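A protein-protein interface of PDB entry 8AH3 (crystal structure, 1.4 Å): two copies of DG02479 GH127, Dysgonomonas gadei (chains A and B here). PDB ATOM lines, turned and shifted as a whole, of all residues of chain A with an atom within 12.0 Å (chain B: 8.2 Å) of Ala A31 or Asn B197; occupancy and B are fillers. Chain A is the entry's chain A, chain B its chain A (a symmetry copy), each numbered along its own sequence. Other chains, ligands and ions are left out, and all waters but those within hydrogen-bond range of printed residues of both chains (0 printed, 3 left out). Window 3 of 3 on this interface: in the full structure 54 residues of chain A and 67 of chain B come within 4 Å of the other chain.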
ATOM      1  N   SER A  26      11.280  -7.567 -34.046  1.00  0.00           N
ATOM      2  CA  SER A  26      11.465  -8.241 -32.757  1.00  0.00           C
ATOM      3  C   SER A  26      12.083  -9.599 -33.024  1.00  0.00           C
ATOM      4  O   SER A  26      12.161 -10.042 -34.168  1.00  0.00           O
ATOM      5  CB  SER A  26      10.198  -8.367 -31.986  1.00  0.00           C
ATOM      6  OG  SER A  26       9.370  -9.390 -32.492  1.00  0.00           O
ATOM      7  N   SER A  27      12.500 -10.266 -31.946  1.00  0.00           N
ATOM      8  CA  SER A  27      13.031 -11.616 -32.007  1.00  0.00           C
ATOM      9  C   SER A  27      11.919 -12.675 -31.932  1.00  0.00           C
ATOM     10  O   SER A  27      12.190 -13.852 -31.720  1.00  0.00           O
ATOM     11  CB  SER A  27      14.145 -11.769 -30.973  1.00  0.00           C
ATOM     12  OG  SER A  27      13.679 -11.519 -29.648  1.00  0.00           O
ATOM     13  N   ASN A  28      10.633 -12.311 -32.095  1.00  0.00           N
ATOM     14  CA  ASN A  28       9.558 -13.300 -32.108  1.00  0.00           C
ATOM     15  C   ASN A  28       9.899 -14.497 -33.029  1.00  0.00           C
ATOM     16  O   ASN A  28      10.416 -14.303 -34.119  1.00  0.00           O
ATOM     17  CB  ASN A  28       8.263 -12.661 -32.582  1.00  0.00           C
ATOM     18  CG  ASN A  28       7.110 -13.616 -32.634  1.00  0.00           C
ATOM     19  OD1 ASN A  28       6.428 -13.888 -31.633  1.00  0.00           O
ATOM     20  ND2 ASN A  28       6.879 -14.120 -33.828  1.00  0.00           N
ATOM     21  N   ASP A  29       9.577 -15.714 -32.554  1.00  0.00           N
ATOM     22  CA  ASP A  29       9.817 -16.957 -33.298  1.00  0.00           C
ATOM     23  C   ASP A  29       8.784 -17.035 -34.419  1.00  0.00           C
ATOM     24  O   ASP A  29       7.603 -17.222 -34.159  1.00  0.00           O
ATOM     25  CB  ASP A  29       9.655 -18.164 -32.363  1.00  0.00           C
ATOM     26  CG  ASP A  29       9.899 -19.540 -32.994  1.00  0.00           C
ATOM     27  OD1 ASP A  29       9.942 -19.631 -34.240  1.00  0.00           O
ATOM     28  OD2 ASP A  29      10.083 -20.500 -32.217  1.00  0.00           O
ATOM     29  N   PRO A  30       9.177 -16.906 -35.706  1.00  0.00           N
ATOM     30  CA  PRO A  30       8.181 -16.906 -36.787  1.00  0.00           C
ATOM     31  C   PRO A  30       7.429 -18.239 -36.936  1.00  0.00           C
ATOM     32  O   PRO A  30       6.292 -18.237 -37.402  1.00  0.00           O
ATOM     33  CB  PRO A  30       8.989 -16.507 -38.021  1.00  0.00           C
ATOM     34  CG  PRO A  30      10.414 -16.908 -37.705  1.00  0.00           C
ATOM     35  CD  PRO A  30      10.554 -16.718 -36.199  1.00  0.00           C
ATOM     36  N   ALA A  31       8.000 -19.347 -36.430  1.00  0.00           N
ATOM     37  CA  ALA A  31       7.324 -20.644 -36.483  1.00  0.00           C
ATOM     38  C   ALA A  31       6.275 -20.784 -35.391  1.00  0.00           C
ATOM     39  O   ALA A  31       5.625 -21.825 -35.312  1.00  0.00           O
ATOM     40  CB  ALA A  31       8.335 -21.769 -36.425  1.00  0.00           C
ATOM     41  N   GLY A  32       6.127 -19.789 -34.472  1.00  0.00           N
ATOM     42  CA  GLY A  32       5.094 -19.897 -33.466  1.00  0.00           C
ATOM     43  C   GLY A  32       5.556 -20.451 -32.111  1.00  0.00           C
ATOM     44  O   GLY A  32       4.724 -20.633 -31.218  1.00  0.00           O
ATOM     45  N   GLY A  33       6.835 -20.756 -31.996  1.00  0.00           N
ATOM     46  CA  GLY A  33       7.298 -21.532 -30.858  1.00  0.00           C
ATOM     47  C   GLY A  33       7.927 -20.648 -29.779  1.00  0.00           C
ATOM     48  O   GLY A  33       7.598 -19.463 -29.650  1.00  0.00           O
ATOM     49  N   VAL A  34       8.880 -21.246 -29.057  1.00  0.00           N
ATOM     50  CA  VAL A  34       9.431 -20.664 -27.834  1.00  0.00           C
ATOM     51  C   VAL A  34      10.737 -19.963 -28.139  1.00  0.00           C
ATOM     52  O   VAL A  34      11.301 -19.320 -27.230  1.00  0.00           O
ATOM     53  CB  VAL A  34       9.668 -21.737 -26.739  1.00  0.00           C
ATOM     54  CG1 VAL A  34       8.395 -22.386 -26.322  1.00  0.00           C
ATOM     55  CG2 VAL A  34      10.756 -22.756 -27.145  1.00  0.00           C
ATOM     56  N   LEU A  35      11.265 -20.040 -29.373  1.00  0.00           N
ATOM     57  CA  LEU A  35      12.581 -19.472 -29.677  1.00  0.00           C
ATOM     58  C   LEU A  35      12.439 -17.993 -30.057  1.00  0.00           C
ATOM     59  O   LEU A  35      12.774 -17.555 -31.168  1.00  0.00           O
ATOM     60  CB  LEU A  35      13.293 -20.233 -30.804  1.00  0.00           C
ATOM     61  CG  LEU A  35      13.622 -21.702 -30.513  1.00  0.00           C
ATOM     62  CD1 LEU A  35      14.263 -22.335 -31.744  1.00  0.00           C
ATOM     63  CD2 LEU A  35      14.526 -21.834 -29.301  1.00  0.00           C
ATOM     64  N   ASP A  36      11.932 -17.224 -29.083  1.00  0.00           N
ATOM     65  CA  ASP A  36      11.585 -15.813 -29.259  1.00  0.00           C
ATOM     66  C   ASP A  36      12.773 -14.902 -29.016  1.00  0.00           C
ATOM     67  O   ASP A  36      12.619 -13.759 -28.574  1.00  0.00           O
ATOM     68  CB  ASP A  36      10.406 -15.470 -28.353  1.00  0.00           C
ATOM     69  CG  ASP A  36       9.119 -16.189 -28.664  1.00  0.00           C
ATOM     70  OD1 ASP A  36       8.737 -16.254 -29.910  1.00  0.00           O
ATOM     71  OD2 ASP A  36       8.464 -16.681 -27.747  1.00  0.00           O
ATOM     72  N   HIS A  37      13.965 -15.367 -29.377  1.00  0.00           N
ATOM     73  CA  HIS A  37      15.240 -14.702 -29.196  1.00  0.00           C
ATOM     74  C   HIS A  37      16.140 -15.059 -30.372  1.00  0.00           C
ATOM     75  O   HIS A  37      15.978 -16.163 -30.901  1.00  0.00           O
ATOM     76  CB  HIS A  37      15.914 -15.097 -27.858  1.00  0.00           C
ATOM     77  CG  HIS A  37      16.017 -16.586 -27.656  1.00  0.00           C
ATOM     78  ND1 HIS A  37      17.043 -17.337 -28.197  1.00  0.00           N
ATOM     79  CD2 HIS A  37      15.128 -17.468 -27.096  1.00  0.00           C
ATOM     80  CE1 HIS A  37      16.788 -18.628 -27.903  1.00  0.00           C
ATOM     81  NE2 HIS A  37      15.640 -18.725 -27.200  1.00  0.00           N
ATOM     82  N   LEU A  38      17.102 -14.198 -30.697  1.00  0.00           N
ATOM     83  CA  LEU A  38      18.262 -14.577 -31.481  1.00  0.00           C
ATOM     84  C   LEU A  38      19.134 -15.461 -30.602  1.00  0.00           C
ATOM     85  O   LEU A  38      19.075 -15.384 -29.353  1.00  0.00           O
ATOM     86  CB  LEU A  38      19.065 -13.380 -31.991  1.00  0.00           C
ATOM     87  CG  LEU A  38      18.263 -12.267 -32.673  1.00  0.00           C
ATOM     88  CD1 LEU A  38      19.188 -11.176 -33.201  1.00  0.00           C
ATOM     89  CD2 LEU A  38      17.313 -12.794 -33.757  1.00  0.00           C
ATOM     90  N   GLU B 184      -3.372 -30.879 -24.157  1.00  0.00           N
ATOM     91  CA  GLU B 184      -2.287 -31.731 -23.687  1.00  0.00           C
ATOM     92  C   GLU B 184      -1.807 -31.338 -22.272  1.00  0.00           C
ATOM     93  O   GLU B 184      -0.885 -31.957 -21.744  1.00  0.00           O
ATOM     94  CB  GLU B 184      -1.116 -31.722 -24.664  1.00  0.00           C
ATOM     95  CG  GLU B 184      -0.491 -30.361 -24.950  1.00  0.00           C
ATOM     96  CD  GLU B 184      -1.165 -29.463 -25.978  1.00  0.00           C
ATOM     97  OE1 GLU B 184      -2.401 -29.563 -26.184  1.00  0.00           O
ATOM     98  OE2 GLU B 184      -0.453 -28.646 -26.544  1.00  0.00           O
ATOM     99  N   THR B 187       1.871 -27.224 -20.556  1.00  0.00           N
ATOM    100  CA  THR B 187       3.193 -27.568 -21.020  1.00  0.00           C
ATOM    101  C   THR B 187       4.244 -26.463 -20.876  1.00  0.00           C
ATOM    102  O   THR B 187       5.349 -26.573 -21.358  1.00  0.00           O
ATOM    103  CB  THR B 187       3.066 -27.999 -22.484  1.00  0.00           C
ATOM    104  OG1 THR B 187       2.472 -26.890 -23.169  1.00  0.00           O
ATOM    105  CG2 THR B 187       2.205 -29.238 -22.606  1.00  0.00           C
ATOM    106  N   LYS B 194       6.159 -31.943 -24.386  1.00  0.00           N
ATOM    107  CA  LYS B 194       6.462 -31.101 -25.539  1.00  0.00           C
ATOM    108  C   LYS B 194       5.492 -29.922 -25.651  1.00  0.00           C
ATOM    109  O   LYS B 194       4.308 -30.021 -25.353  1.00  0.00           O
ATOM    110  CB  LYS B 194       6.386 -31.958 -26.814  1.00  0.00           C
ATOM    111  CG  LYS B 194       7.475 -33.018 -26.871  1.00  0.00           C
ATOM    112  CD  LYS B 194       7.465 -33.913 -28.095  1.00  0.00           C
ATOM    113  CE  LYS B 194       8.539 -34.979 -27.989  1.00  0.00           C
ATOM    114  NZ  LYS B 194       8.464 -35.968 -29.092  1.00  0.00           N
ATOM    115  N   GLN B 195       6.020 -28.778 -26.098  1.00  0.00           N
ATOM    116  CA  GLN B 195       5.210 -27.577 -26.286  1.00  0.00           C
ATOM    117  C   GLN B 195       4.785 -27.411 -27.747  1.00  0.00           C
ATOM    118  O   GLN B 195       5.553 -27.735 -28.623  1.00  0.00           O
ATOM    119  CB  GLN B 195       6.016 -26.346 -25.922  1.00  0.00           C
ATOM    120  CG  GLN B 195       6.506 -26.409 -24.477  1.00  0.00           C
ATOM    121  CD  GLN B 195       7.378 -25.216 -24.169  1.00  0.00           C
ATOM    122  OE1 GLN B 195       8.588 -25.234 -24.383  1.00  0.00           O
ATOM    123  NE2 GLN B 195       6.745 -24.198 -23.611  1.00  0.00           N
ATOM    124  N   ASP B 196       3.555 -26.922 -27.924  1.00  0.00           N
ATOM    125  CA  ASP B 196       2.964 -26.630 -29.232  1.00  0.00           C
ATOM    126  C   ASP B 196       3.437 -25.276 -29.775  1.00  0.00           C
ATOM    127  O   ASP B 196       4.031 -24.464 -29.056  1.00  0.00           O
ATOM    128  CB  ASP B 196       1.442 -26.623 -29.125  1.00  0.00           C
ATOM    129  CG  ASP B 196       0.705 -26.873 -30.443  1.00  0.00           C
ATOM    130  OD1 ASP B 196       1.365 -27.116 -31.469  1.00  0.00           O
ATOM    131  OD2 ASP B 196      -0.518 -26.821 -30.421  1.00  0.00           O
ATOM    132  N   ASN B 197       3.190 -25.064 -31.086  1.00  0.00           N
ATOM    133  CA  ASN B 197       3.318 -23.756 -31.717  1.00  0.00           C
ATOM    134  C   ASN B 197       1.990 -22.991 -31.696  1.00  0.00           C
ATOM    135  O   ASN B 197       0.888 -23.540 -31.581  1.00  0.00           O
ATOM    136  CB  ASN B 197       3.825 -23.888 -33.151  1.00  0.00           C
ATOM    137  CG  ASN B 197       5.230 -24.412 -33.268  1.00  0.00           C
ATOM    138  OD1 ASN B 197       6.134 -24.038 -32.526  1.00  0.00           O
ATOM    139  ND2 ASN B 197       5.436 -25.300 -34.232  1.00  0.00           N
ATOM    140  N   ASN B 198       2.079 -21.650 -31.847  1.00  0.00           N
ATOM    141  CA  ASN B 198       0.919 -20.787 -31.977  1.00  0.00           C
ATOM    142  C   ASN B 198       1.261 -19.729 -33.028  1.00  0.00           C
ATOM    143  O   ASN B 198       1.869 -18.696 -32.718  1.00  0.00           O
ATOM    144  CB  ASN B 198       0.588 -20.102 -30.649  1.00  0.00           C
ATOM    145  CG  ASN B 198      -0.476 -19.040 -30.768  1.00  0.00           C
ATOM    146  OD1 ASN B 198      -1.330 -19.113 -31.665  1.00  0.00           O
ATOM    147  ND2 ASN B 198      -0.477 -18.076 -29.840  1.00  0.00           N
ATOM    148  N   THR B 199       0.895 -19.994 -34.296  1.00  0.00           N
ATOM    149  CA  THR B 199       1.203 -19.053 -35.345  1.00  0.00           C
ATOM    150  C   THR B 199       0.002 -18.140 -35.606  1.00  0.00           C
ATOM    151  O   THR B 199       0.183 -17.149 -36.298  1.00  0.00           O
ATOM    152  CB  THR B 199       1.619 -19.756 -36.657  1.00  0.00           C
ATOM    153  OG1 THR B 199       0.486 -20.543 -36.995  1.00  0.00           O
ATOM    154  CG2 THR B 199       2.872 -20.594 -36.554  1.00  0.00           C
ATOM    155  N   THR B 200      -1.184 -18.433 -35.056  1.00  0.00           N
ATOM    156  CA  THR B 200      -2.392 -17.698 -35.417  1.00  0.00           C
ATOM    157  C   THR B 200      -2.783 -16.645 -34.385  1.00  0.00           C
ATOM    158  O   THR B 200      -3.376 -15.616 -34.712  1.00  0.00           O
ATOM    159  CB  THR B 200      -3.584 -18.634 -35.584  1.00  0.00           C
ATOM    160  OG1 THR B 200      -3.906 -19.247 -34.332  1.00  0.00           O
ATOM    161  CG2 THR B 200      -3.326 -19.689 -36.648  1.00  0.00           C
ATOM    162  N   GLY B 201      -2.512 -16.935 -33.096  1.00  0.00           N
ATOM    163  CA  GLY B 201      -3.039 -16.068 -32.057  1.00  0.00           C
ATOM    164  C   GLY B 201      -4.499 -16.326 -31.708  1.00  0.00           C
ATOM    165  O   GLY B 201      -5.087 -15.619 -30.874  1.00  0.00           O
ATOM    166  N   ARG B 203      -6.239 -18.424 -29.857  1.00  0.00           N
ATOM    167  CA  ARG B 203      -6.691 -18.706 -28.505  1.00  0.00           C
ATOM    168  C   ARG B 203      -6.086 -17.715 -27.496  1.00  0.00           C
ATOM    169  O   ARG B 203      -6.190 -17.914 -26.303  1.00  0.00           O
ATOM    170  CB  ARG B 203      -6.255 -20.118 -28.108  1.00  0.00           C
ATOM    171  CG  ARG B 203      -6.970 -21.259 -28.832  1.00  0.00           C
ATOM    172  CD  ARG B 203      -6.255 -22.565 -28.471  1.00  0.00           C
ATOM    173  NE  ARG B 203      -6.433 -23.026 -27.086  1.00  0.00           N
ATOM    174  CZ  ARG B 203      -5.523 -23.084 -26.087  1.00  0.00           C
ATOM    175  NH1 ARG B 203      -4.299 -23.541 -26.273  1.00  0.00           N
ATOM    176  NH2 ARG B 203      -5.899 -22.833 -24.844  1.00  0.00           N
ATOM    177  N   PHE B 237       0.472  -9.831 -29.444  1.00  0.00           N
ATOM    178  CA  PHE B 237       0.105  -9.747 -30.864  1.00  0.00           C
ATOM    179  C   PHE B 237      -0.778  -8.507 -31.043  1.00  0.00           C
ATOM    180  O   PHE B 237      -1.766  -8.336 -30.334  1.00  0.00           O
ATOM    181  CB  PHE B 237      -0.799 -10.939 -31.264  1.00  0.00           C
ATOM    182  CG  PHE B 237      -0.158 -12.290 -31.441  1.00  0.00           C
ATOM    183  CD1 PHE B 237       0.522 -12.913 -30.404  1.00  0.00           C
ATOM    184  CD2 PHE B 237      -0.428 -13.048 -32.561  1.00  0.00           C
ATOM    185  CE1 PHE B 237       1.080 -14.176 -30.546  1.00  0.00           C
ATOM    186  CE2 PHE B 237       0.089 -14.327 -32.683  1.00  0.00           C
ATOM    187  CZ  PHE B 237       0.803 -14.907 -31.669  1.00  0.00           C
ATOM    188  N   GLU B 309      -0.647 -14.172 -25.504  1.00  0.00           N
ATOM    189  CA  GLU B 309      -0.764 -15.583 -25.148  1.00  0.00           C
ATOM    190  C   GLU B 309      -0.872 -15.705 -23.616  1.00  0.00           C
ATOM    191  O   GLU B 309      -0.207 -14.935 -22.898  1.00  0.00           O
ATOM    192  CB  GLU B 309       0.437 -16.350 -25.619  1.00  0.00           C
ATOM    193  CG  GLU B 309       0.759 -16.287 -27.094  1.00  0.00           C
ATOM    194  CD  GLU B 309       1.995 -17.083 -27.410  1.00  0.00           C
ATOM    195  OE1 GLU B 309       3.056 -16.792 -26.869  1.00  0.00           O
ATOM    196  OE2 GLU B 309       1.904 -18.054 -28.230  1.00  0.00           O
ATOM    197  N   HIS B 312       3.068 -19.726 -22.867  1.00  0.00           N
ATOM    198  CA  HIS B 312       3.528 -20.038 -24.217  1.00  0.00           C
ATOM    199  C   HIS B 312       2.465 -20.859 -24.955  1.00  0.00           C
ATOM    200  O   HIS B 312       1.910 -21.840 -24.421  1.00  0.00           O
ATOM    201  CB  HIS B 312       4.860 -20.781 -24.261  1.00  0.00           C
ATOM    202  CG  HIS B 312       5.122 -21.253 -25.656  1.00  0.00           C
ATOM    203  ND1 HIS B 312       5.467 -20.392 -26.686  1.00  0.00           N
ATOM    204  CD2 HIS B 312       4.868 -22.485 -26.193  1.00  0.00           C
ATOM    205  CE1 HIS B 312       5.459 -21.086 -27.835  1.00  0.00           C
ATOM    206  NE2 HIS B 312       5.077 -22.382 -27.546  1.00  0.00           N
ATOM    207  N   ALA B 313       2.097 -20.383 -26.175  1.00  0.00           N
ATOM    208  CA  ALA B 313       1.011 -21.002 -26.935  1.00  0.00           C
ATOM    209  C   ALA B 313      -0.238 -21.266 -26.117  1.00  0.00           C
ATOM    210  O   ALA B 313      -0.953 -22.261 -26.356  1.00  0.00           O
ATOM    211  CB  ALA B 313       1.514 -22.292 -27.568  1.00  0.00           C
ATOM    212  N   ASN B 314      -0.621 -20.357 -25.195  1.00  0.00           N
ATOM    213  CA  ASN B 314      -1.889 -20.425 -24.499  1.00  0.00           C
ATOM    214  C   ASN B 314      -2.076 -21.739 -23.719  1.00  0.00           C
ATOM    215  O   ASN B 314      -3.213 -22.194 -23.533  1.00  0.00           O
ATOM    216  CB  ASN B 314      -3.016 -20.193 -25.504  1.00  0.00           C
ATOM    217  CG  ASN B 314      -2.897 -18.840 -26.156  1.00  0.00           C
ATOM    218  OD1 ASN B 314      -2.944 -17.841 -25.422  1.00  0.00           O
ATOM    219  ND2 ASN B 314      -2.858 -18.797 -27.504  1.00  0.00           N
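O of Gly A32 is in hydrogen-bond range of N of Asn B198. The backbone NH (N) of Gly A33 lies close to the side-chain amide oxygen (OD1) of Asn B197, 3.4 Å away.
Gly A32 touches just these residues of chain B: Asn B197, Asn B198, Thr B199 and His B312. Of the printed residues of chain B, Gly A33 touches Asn B197 and His B312. Printed residues of chain B within 4 Å of Val A34: Gln B195 and His B312. Printed residues of chain A within 4 Å of Gln B195: Val A34. No residue of chain A comes within 4 Å of Asp B196. Of chain A, only Ala A31 (3.3 Å), Gly A32 (3.5 Å) and Gly A33 (3.2 Å) come within 4 Å of Asn B197. Asn B198 touches just one residue of chain A: Gly A32. Of chain A, only Ala A31 (3.3 Å) and Gly A32 (3.9 Å) come within 4 Å of Thr B199. Of the printed residues of chain A, His B312 touches Gly A32 (3.5 Å), Gly A33 (3.2 Å) and Val A34 (3.5 Å). The nearest residue of chain B that does not touch Ala A31 is Asn B198 (5.0 Å). The nearest printed residue of chain A that does not touch His B312 is Asp A36 (4.9 Å).
Of the 13 printed residues of chain A, 4 touch a printed residue of chain B. Hydrophobic or aromatic side chains of chain A within 4 Å of the printed part of chain B: Val A34. Among the printed residues, 10 pairs touch across the chains.
Ala A31 touches Asn B197 (O to CG, 3.3 Å). Thr B199 touches Ala A31. O of Gly A32 touches CA of Asn B197, 3.5 Å away. CA of Gly A32 touches CG2 of Thr B199 (3.9 Å). Gly A32 touches His B312 (O to CE1, 3.5 Å). C of Gly A33 touches CE1 of His B312 (3.2 Å). CG1 of Val A34 touches OE1 of Gln B195 (3.5 Å). Val A34 touches His B312 (CG1 to CG, 3.5 Å).
No position is printed for both chains.
The side-chain carboxylate (OD1) of Asp A29 lies within hydrogen-bond range of the backbone NH (N) of Ala A31. The backbone NH (N) of Val A34 sits at hydrogen-bond distance from the side-chain carboxylate (OD2) of Asp A29 (3.5 Å). O of Asp B196 is in hydrogen-bond range of NE2 of His B312 (2.8 Å). OD1 of Asn B198 sits close to N of Thr B200, at 3.5 Å. OE2 of Glu B309 sits at hydrogen-bond distance from ND2 of Asn B198 (2.9 Å). The side-chain amide nitrogen (ND2) of Asn B198 sits close to the side-chain amide nitrogen (ND2) of Asn B314 (3.4 Å).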
